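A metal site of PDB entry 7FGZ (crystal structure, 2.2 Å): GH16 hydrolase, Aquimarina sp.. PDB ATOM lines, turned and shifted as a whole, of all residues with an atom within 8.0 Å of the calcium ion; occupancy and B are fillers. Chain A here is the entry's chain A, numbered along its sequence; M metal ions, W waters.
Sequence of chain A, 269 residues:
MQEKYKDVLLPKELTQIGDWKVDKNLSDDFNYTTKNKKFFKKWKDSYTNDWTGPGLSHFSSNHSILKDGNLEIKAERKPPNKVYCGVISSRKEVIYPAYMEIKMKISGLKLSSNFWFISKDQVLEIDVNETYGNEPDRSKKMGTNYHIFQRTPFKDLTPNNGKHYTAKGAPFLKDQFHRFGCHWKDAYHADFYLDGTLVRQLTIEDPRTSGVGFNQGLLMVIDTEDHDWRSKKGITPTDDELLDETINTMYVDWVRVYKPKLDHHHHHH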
ATOM      1  N   GLN A   2     -20.668   3.136  17.447  1.00  0.00           N
ATOM      2  CA  GLN A   2     -20.393   1.772  17.948  1.00  0.00           C
ATOM      3  C   GLN A   2     -19.075   1.295  17.329  1.00  0.00           C
ATOM      4  O   GLN A   2     -18.002   1.691  17.857  1.00  0.00           O
ATOM      5  CB  GLN A   2     -21.593   0.864  17.655  1.00  0.00           C
ATOM      6  CG  GLN A   2     -21.407  -0.599  18.053  1.00  0.00           C
ATOM      7  CD  GLN A   2     -21.648  -0.792  19.532  1.00  0.00           C
ATOM      8  OE1 GLN A   2     -21.300   0.052  20.354  1.00  0.00           O
ATOM      9  NE2 GLN A   2     -22.294  -1.895  19.860  1.00  0.00           N
ATOM     10  N   GLU A   3     -19.117   0.527  16.230  1.00  0.00           N
ATOM     11  CA  GLU A   3     -17.919  -0.142  15.663  1.00  0.00           C
ATOM     12  C   GLU A   3     -17.554   0.466  14.316  1.00  0.00           C
ATOM     13  O   GLU A   3     -18.457   0.698  13.474  1.00  0.00           O
ATOM     14  CB  GLU A   3     -18.148  -1.642  15.478  1.00  0.00           C
ATOM     15  CG  GLU A   3     -16.860  -2.441  15.293  1.00  0.00           C
ATOM     16  CD  GLU A   3     -17.136  -3.901  15.042  1.00  0.00           C
ATOM     17  OE1 GLU A   3     -17.891  -4.189  14.078  1.00  0.00           O
ATOM     18  OE2 GLU A   3     -16.636  -4.753  15.822  1.00  0.00           O
ATOM     19  N   LYS A   4     -16.254   0.662  14.123  1.00  0.00           N
ATOM     20  CA  LYS A   4     -15.627   1.051  12.830  1.00  0.00           C
ATOM     21  C   LYS A   4     -14.912  -0.186  12.265  1.00  0.00           C
ATOM     22  O   LYS A   4     -14.350  -0.970  13.056  1.00  0.00           O
ATOM     23  CB  LYS A   4     -14.662   2.210  13.068  1.00  0.00           C
ATOM     24  CG  LYS A   4     -15.229   3.380  13.840  1.00  0.00           C
ATOM     25  CD  LYS A   4     -14.934   4.700  13.212  1.00  0.00           C
ATOM     26  CE  LYS A   4     -13.481   5.089  13.323  1.00  0.00           C
ATOM     27  NZ  LYS A   4     -13.016   5.081  14.734  1.00  0.00           N
ATOM     28  N   TYR A   5     -14.911  -0.365  10.944  1.00  0.00           N
ATOM     29  CA  TYR A   5     -14.334  -1.576  10.323  1.00  0.00           C
ATOM     30  C   TYR A   5     -12.819  -1.654  10.600  1.00  0.00           C
ATOM     31  O   TYR A   5     -12.330  -2.775  10.694  1.00  0.00           O
ATOM     32  CB  TYR A   5     -14.691  -1.640   8.842  1.00  0.00           C
ATOM     33  CG  TYR A   5     -14.048  -0.591   7.971  1.00  0.00           C
ATOM     34  CD1 TYR A   5     -12.707  -0.685   7.603  1.00  0.00           C
ATOM     35  CD2 TYR A   5     -14.774   0.484   7.515  1.00  0.00           C
ATOM     36  CE1 TYR A   5     -12.101   0.314   6.851  1.00  0.00           C
ATOM     37  CE2 TYR A   5     -14.209   1.443   6.698  1.00  0.00           C
ATOM     38  CZ  TYR A   5     -12.867   1.374   6.395  1.00  0.00           C
ATOM     39  OH  TYR A   5     -12.319   2.345   5.607  1.00  0.00           O
ATOM     40  N   ASP A  28     -16.264   1.162   3.587  1.00  0.00           N
ATOM     41  CA  ASP A  28     -17.206   2.180   4.119  1.00  0.00           C
ATOM     42  C   ASP A  28     -17.770   1.737   5.457  1.00  0.00           C
ATOM     43  O   ASP A  28     -18.305   0.611   5.548  1.00  0.00           O
ATOM     44  CB  ASP A  28     -18.344   2.430   3.139  1.00  0.00           C
ATOM     45  CG  ASP A  28     -18.792   3.896   3.151  1.00  0.00           C
ATOM     46  OD1 ASP A  28     -18.881   4.475   4.250  1.00  0.00           O
ATOM     47  OD2 ASP A  28     -19.025   4.445   2.055  1.00  0.00           O
ATOM     48  N   ASP A  29     -17.691   2.603   6.454  1.00  0.00           N
ATOM     49  CA  ASP A  29     -18.422   2.458   7.737  1.00  0.00           C
ATOM     50  C   ASP A  29     -19.915   2.820   7.565  1.00  0.00           C
ATOM     51  O   ASP A  29     -20.677   2.615   8.545  1.00  0.00           O
ATOM     52  CB  ASP A  29     -17.769   3.308   8.827  1.00  0.00           C
ATOM     53  CG  ASP A  29     -16.596   2.582   9.452  1.00  0.00           C
ATOM     54  OD1 ASP A  29     -16.782   1.396   9.863  1.00  0.00           O
ATOM     55  OD2 ASP A  29     -15.493   3.201   9.481  1.00  0.00           O
ATOM     56  N   PHE A  30     -20.328   3.364   6.411  1.00  0.00           N
ATOM     57  CA  PHE A  30     -21.751   3.689   6.134  1.00  0.00           C
ATOM     58  C   PHE A  30     -22.346   4.478   7.303  1.00  0.00           C
ATOM     59  O   PHE A  30     -23.548   4.279   7.680  1.00  0.00           O
ATOM     60  CB  PHE A  30     -22.540   2.385   5.892  1.00  0.00           C
ATOM     61  CG  PHE A  30     -22.143   1.689   4.624  1.00  0.00           C
ATOM     62  CD1 PHE A  30     -22.148   2.371   3.418  1.00  0.00           C
ATOM     63  CD2 PHE A  30     -21.751   0.367   4.630  1.00  0.00           C
ATOM     64  CE1 PHE A  30     -21.774   1.721   2.244  1.00  0.00           C
ATOM     65  CE2 PHE A  30     -21.404  -0.277   3.451  1.00  0.00           C
ATOM     66  CZ  PHE A  30     -21.407   0.406   2.276  1.00  0.00           C
ATOM     67  N   ASN A  31     -21.552   5.374   7.893  1.00  0.00           N
ATOM     68  CA  ASN A  31     -21.974   6.186   9.058  1.00  0.00           C
ATOM     69  C   ASN A  31     -22.482   7.558   8.562  1.00  0.00           C
ATOM     70  O   ASN A  31     -22.932   8.335   9.398  1.00  0.00           O
ATOM     71  CB  ASN A  31     -20.871   6.277  10.117  1.00  0.00           C
ATOM     72  CG  ASN A  31     -20.564   4.962  10.817  1.00  0.00           C
ATOM     73  OD1 ASN A  31     -21.354   4.011  10.807  1.00  0.00           O
ATOM     74  ND2 ASN A  31     -19.405   4.907  11.436  1.00  0.00           N
ATOM     75  N   TYR A  32     -22.460   7.831   7.255  1.00  0.00           N
ATOM     76  CA  TYR A  32     -23.199   8.970   6.650  1.00  0.00           C
ATOM     77  C   TYR A  32     -24.663   8.979   7.125  1.00  0.00           C
ATOM     78  O   TYR A  32     -25.256   7.899   7.262  1.00  0.00           O
ATOM     79  CB  TYR A  32     -23.302   8.850   5.120  1.00  0.00           C
ATOM     80  CG  TYR A  32     -22.076   8.369   4.399  1.00  0.00           C
ATOM     81  CD1 TYR A  32     -20.930   9.128   4.333  1.00  0.00           C
ATOM     82  CD2 TYR A  32     -22.104   7.152   3.716  1.00  0.00           C
ATOM     83  CE1 TYR A  32     -19.826   8.696   3.614  1.00  0.00           C
ATOM     84  CE2 TYR A  32     -21.007   6.703   3.015  1.00  0.00           C
ATOM     85  CZ  TYR A  32     -19.849   7.471   2.972  1.00  0.00           C
ATOM     86  OH  TYR A  32     -18.761   7.040   2.261  1.00  0.00           O
ATOM     87  N   LEU A  66     -29.429   5.367   4.017  1.00  0.00           N
ATOM     88  CA  LEU A  66     -28.435   5.530   5.105  1.00  0.00           C
ATOM     89  C   LEU A  66     -29.150   5.932   6.403  1.00  0.00           C
ATOM     90  O   LEU A  66     -29.933   6.873   6.370  1.00  0.00           O
ATOM     91  CB  LEU A  66     -27.360   6.529   4.675  1.00  0.00           C
ATOM     92  CG  LEU A  66     -26.196   5.931   3.885  1.00  0.00           C
ATOM     93  CD1 LEU A  66     -25.349   5.016   4.747  1.00  0.00           C
ATOM     94  CD2 LEU A  66     -26.683   5.170   2.665  1.00  0.00           C
ATOM     95  N   LYS A  67     -28.929   5.192   7.481  1.00  0.00           N
ATOM     96  CA  LYS A  67     -29.664   5.397   8.759  1.00  0.00           C
ATOM     97  C   LYS A  67     -28.861   4.794   9.922  1.00  0.00           C
ATOM     98  O   LYS A  67     -28.718   3.531   9.998  1.00  0.00           O
ATOM     99  CB  LYS A  67     -31.047   4.765   8.650  1.00  0.00           C
ATOM    100  CG  LYS A  67     -32.050   5.196   9.708  1.00  0.00           C
ATOM    101  CD  LYS A  67     -33.475   4.922   9.279  1.00  0.00           C
ATOM    102  CE  LYS A  67     -34.474   5.064  10.413  1.00  0.00           C
ATOM    103  NZ  LYS A  67     -34.212   4.086  11.488  1.00  0.00           N
ATOM    104  N   ASP A  68     -28.410   5.674  10.821  1.00  0.00           N
ATOM    105  CA  ASP A  68     -27.969   5.321  12.191  1.00  0.00           C
ATOM    106  C   ASP A  68     -26.762   4.381  12.146  1.00  0.00           C
ATOM    107  O   ASP A  68     -26.699   3.518  12.990  1.00  0.00           O
ATOM    108  CB  ASP A  68     -29.117   4.688  12.984  1.00  0.00           C
ATOM    109  CG  ASP A  68     -30.325   5.579  13.187  1.00  0.00           C
ATOM    110  OD1 ASP A  68     -30.197   6.848  13.074  1.00  0.00           O
ATOM    111  OD2 ASP A  68     -31.396   5.020  13.420  1.00  0.00           O
ATOM    112  N   GLY A  69     -25.853   4.579  11.194  1.00  0.00           N
ATOM    113  CA  GLY A  69     -24.603   3.803  11.045  1.00  0.00           C
ATOM    114  C   GLY A  69     -24.743   2.566  10.152  1.00  0.00           C
ATOM    115  O   GLY A  69     -23.753   1.841  10.040  1.00  0.00           O
ATOM    116  N   ASN A  70     -25.913   2.346   9.535  1.00  0.00           N
ATOM    117  CA  ASN A  70     -26.139   1.220   8.587  1.00  0.00           C
ATOM    118  C   ASN A  70     -26.479   1.754   7.210  1.00  0.00           C
ATOM    119  O   ASN A  70     -27.189   2.818   7.105  1.00  0.00           O
ATOM    120  CB  ASN A  70     -27.211   0.261   9.085  1.00  0.00           C
ATOM    121  CG  ASN A  70     -26.830  -0.366  10.416  1.00  0.00           C
ATOM    122  OD1 ASN A  70     -25.736  -0.920  10.564  1.00  0.00           O
ATOM    123  ND2 ASN A  70     -27.711  -0.240  11.396  1.00  0.00           N
ATOM    124  N   LEU A  71     -25.980   1.058   6.189  1.00  0.00           N
ATOM    125  CA  LEU A  71     -26.664   0.939   4.882  1.00  0.00           C
ATOM    126  C   LEU A  71     -27.821  -0.033   5.103  1.00  0.00           C
ATOM    127  O   LEU A  71     -27.587  -1.134   5.549  1.00  0.00           O
ATOM    128  CB  LEU A  71     -25.695   0.459   3.800  1.00  0.00           C
ATOM    129  CG  LEU A  71     -26.348  -0.053   2.508  1.00  0.00           C
ATOM    130  CD1 LEU A  71     -27.072   1.071   1.801  1.00  0.00           C
ATOM    131  CD2 LEU A  71     -25.334  -0.682   1.580  1.00  0.00           C
ATOM    132  N   LYS A 103     -19.972  -6.658   7.098  1.00  0.00           N
ATOM    133  CA  LYS A 103     -20.664  -6.923   8.363  1.00  0.00           C
ATOM    134  C   LYS A 103     -22.138  -6.658   8.099  1.00  0.00           C
ATOM    135  O   LYS A 103     -22.501  -5.487   7.842  1.00  0.00           O
ATOM    136  CB  LYS A 103     -20.087  -6.015   9.445  1.00  0.00           C
ATOM    137  CG  LYS A 103     -20.694  -6.219  10.828  1.00  0.00           C
ATOM    138  CD  LYS A 103     -20.173  -5.253  11.835  1.00  0.00           C
ATOM    139  CE  LYS A 103     -20.859  -5.416  13.177  1.00  0.00           C
ATOM    140  NZ  LYS A 103     -20.582  -4.268  14.076  1.00  0.00           N
ATOM    141  N   PHE A 177     -25.692  -9.061  13.549  1.00  0.00           N
ATOM    142  CA  PHE A 177     -24.597  -8.795  12.572  1.00  0.00           C
ATOM    143  C   PHE A 177     -23.630  -9.974  12.590  1.00  0.00           C
ATOM    144  O   PHE A 177     -23.259 -10.475  13.659  1.00  0.00           O
ATOM    145  CB  PHE A 177     -23.886  -7.483  12.892  1.00  0.00           C
ATOM    146  CG  PHE A 177     -24.729  -6.268  12.667  1.00  0.00           C
ATOM    147  CD1 PHE A 177     -24.970  -5.824  11.381  1.00  0.00           C
ATOM    148  CD2 PHE A 177     -25.297  -5.583  13.735  1.00  0.00           C
ATOM    149  CE1 PHE A 177     -25.750  -4.700  11.157  1.00  0.00           C
ATOM    150  CE2 PHE A 177     -26.074  -4.457  13.501  1.00  0.00           C
ATOM    151  CZ  PHE A 177     -26.304  -4.030  12.215  1.00  0.00           C
ATOM    152  N   VAL A 252     -26.377  -3.292   6.792  1.00  0.00           N
ATOM    153  CA  VAL A 252     -24.913  -3.385   6.553  1.00  0.00           C
ATOM    154  C   VAL A 252     -24.209  -2.330   7.413  1.00  0.00           C
ATOM    155  O   VAL A 252     -24.252  -1.157   7.047  1.00  0.00           O
ATOM    156  CB  VAL A 252     -24.600  -3.166   5.071  1.00  0.00           C
ATOM    157  CG1 VAL A 252     -23.099  -3.099   4.839  1.00  0.00           C
ATOM    158  CG2 VAL A 252     -25.300  -4.218   4.232  1.00  0.00           C
ATOM    159  N   ASP A 253     -23.528  -2.763   8.461  1.00  0.00           N
ATOM    160  CA  ASP A 253     -22.880  -1.831   9.417  1.00  0.00           C
ATOM    161  C   ASP A 253     -21.643  -1.281   8.733  1.00  0.00           C
ATOM    162  O   ASP A 253     -21.399  -0.088   8.829  1.00  0.00           O
ATOM    163  CB  ASP A 253     -22.533  -2.555  10.708  1.00  0.00           C
ATOM    164  CG  ASP A 253     -21.936  -1.621  11.747  1.00  0.00           C
ATOM    165  OD1 ASP A 253     -21.964  -0.388  11.525  1.00  0.00           O
ATOM    166  OD2 ASP A 253     -21.477  -2.122  12.771  1.00  0.00           O
ATOM    167  N   TRP A 254     -20.895  -2.142   8.060  1.00  0.00           N
ATOM    168  CA  TRP A 254     -19.688  -1.736   7.310  1.00  0.00           C
ATOM    169  C   TRP A 254     -19.368  -2.763   6.229  1.00  0.00           C
ATOM    170  O   TRP A 254     -19.895  -3.908   6.298  1.00  0.00           O
ATOM    171  CB  TRP A 254     -18.512  -1.472   8.263  1.00  0.00           C
ATOM    172  CG  TRP A 254     -18.115  -2.504   9.266  1.00  0.00           C
ATOM    173  CD1 TRP A 254     -18.254  -2.396  10.621  1.00  0.00           C
ATOM    174  CD2 TRP A 254     -17.385  -3.728   9.045  1.00  0.00           C
ATOM    175  NE1 TRP A 254     -17.658  -3.451  11.260  1.00  0.00           N
ATOM    176  CE2 TRP A 254     -17.121  -4.290  10.320  1.00  0.00           C
ATOM    177  CE3 TRP A 254     -16.916  -4.409   7.917  1.00  0.00           C
ATOM    178  CZ2 TRP A 254     -16.457  -5.508  10.477  1.00  0.00           C
ATOM    179  CZ3 TRP A 254     -16.240  -5.606   8.069  1.00  0.00           C
ATOM    180  CH2 TRP A 254     -16.014  -6.146   9.339  1.00  0.00           C
ATOM    181  N   VAL A 255     -18.589  -2.327   5.242  1.00  0.00           N
ATOM    182  CA  VAL A 255     -17.888  -3.211   4.278  1.00  0.00           C
ATOM    183  C   VAL A 255     -16.421  -2.802   4.208  1.00  0.00           C
ATOM    184  O   VAL A 255     -16.108  -1.597   4.341  1.00  0.00           O
ATOM    185  CB  VAL A 255     -18.557  -3.198   2.908  1.00  0.00           C
ATOM    186  CG1 VAL A 255     -18.327  -1.888   2.184  1.00  0.00           C
ATOM    187  CG2 VAL A 255     -18.090  -4.378   2.074  1.00  0.00           C
HETATM  188 CA    CA M   1     -21.482   1.644  10.454  1.00  0.00          CA
HETATM  189  O   HOH W   1     -19.120   1.072  11.022  1.00  0.00           O
HETATM  190  O   HOH W   2     -21.824   2.008  12.955  1.00  0.00           O
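The backbone NH of Tyr 5 lies within hydrogen-bond range of the side-chain carboxylate of Asp 29, at 2.8 Å.
OD2 of Asp 253 lies within salt-bridge range of NZ of Lys 103 (2.7 Å).
Water W1 bridges O of Glu 3 and OD1 of Asp 29.
Within 4 Å of the calcium ion: Asp 29, Asn 31, Gly 69 and Asp 253.
The nearest printed residue that does not touch the calcium ion is Phe 30 (4.3 Å).
The calcium ion is bound by O of Asp 29 (2.3 Å), O of Gly 69 (2.3 Å), OD1 of Asp 253 (2.3 Å), O of Asp 253 (2.4 Å), OD1 of Asn 31 (2.4 Å), water W1 (2.5 Å) and water W2 (2.6 Å).
The calcium ion has seven donor atoms within binding distance.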
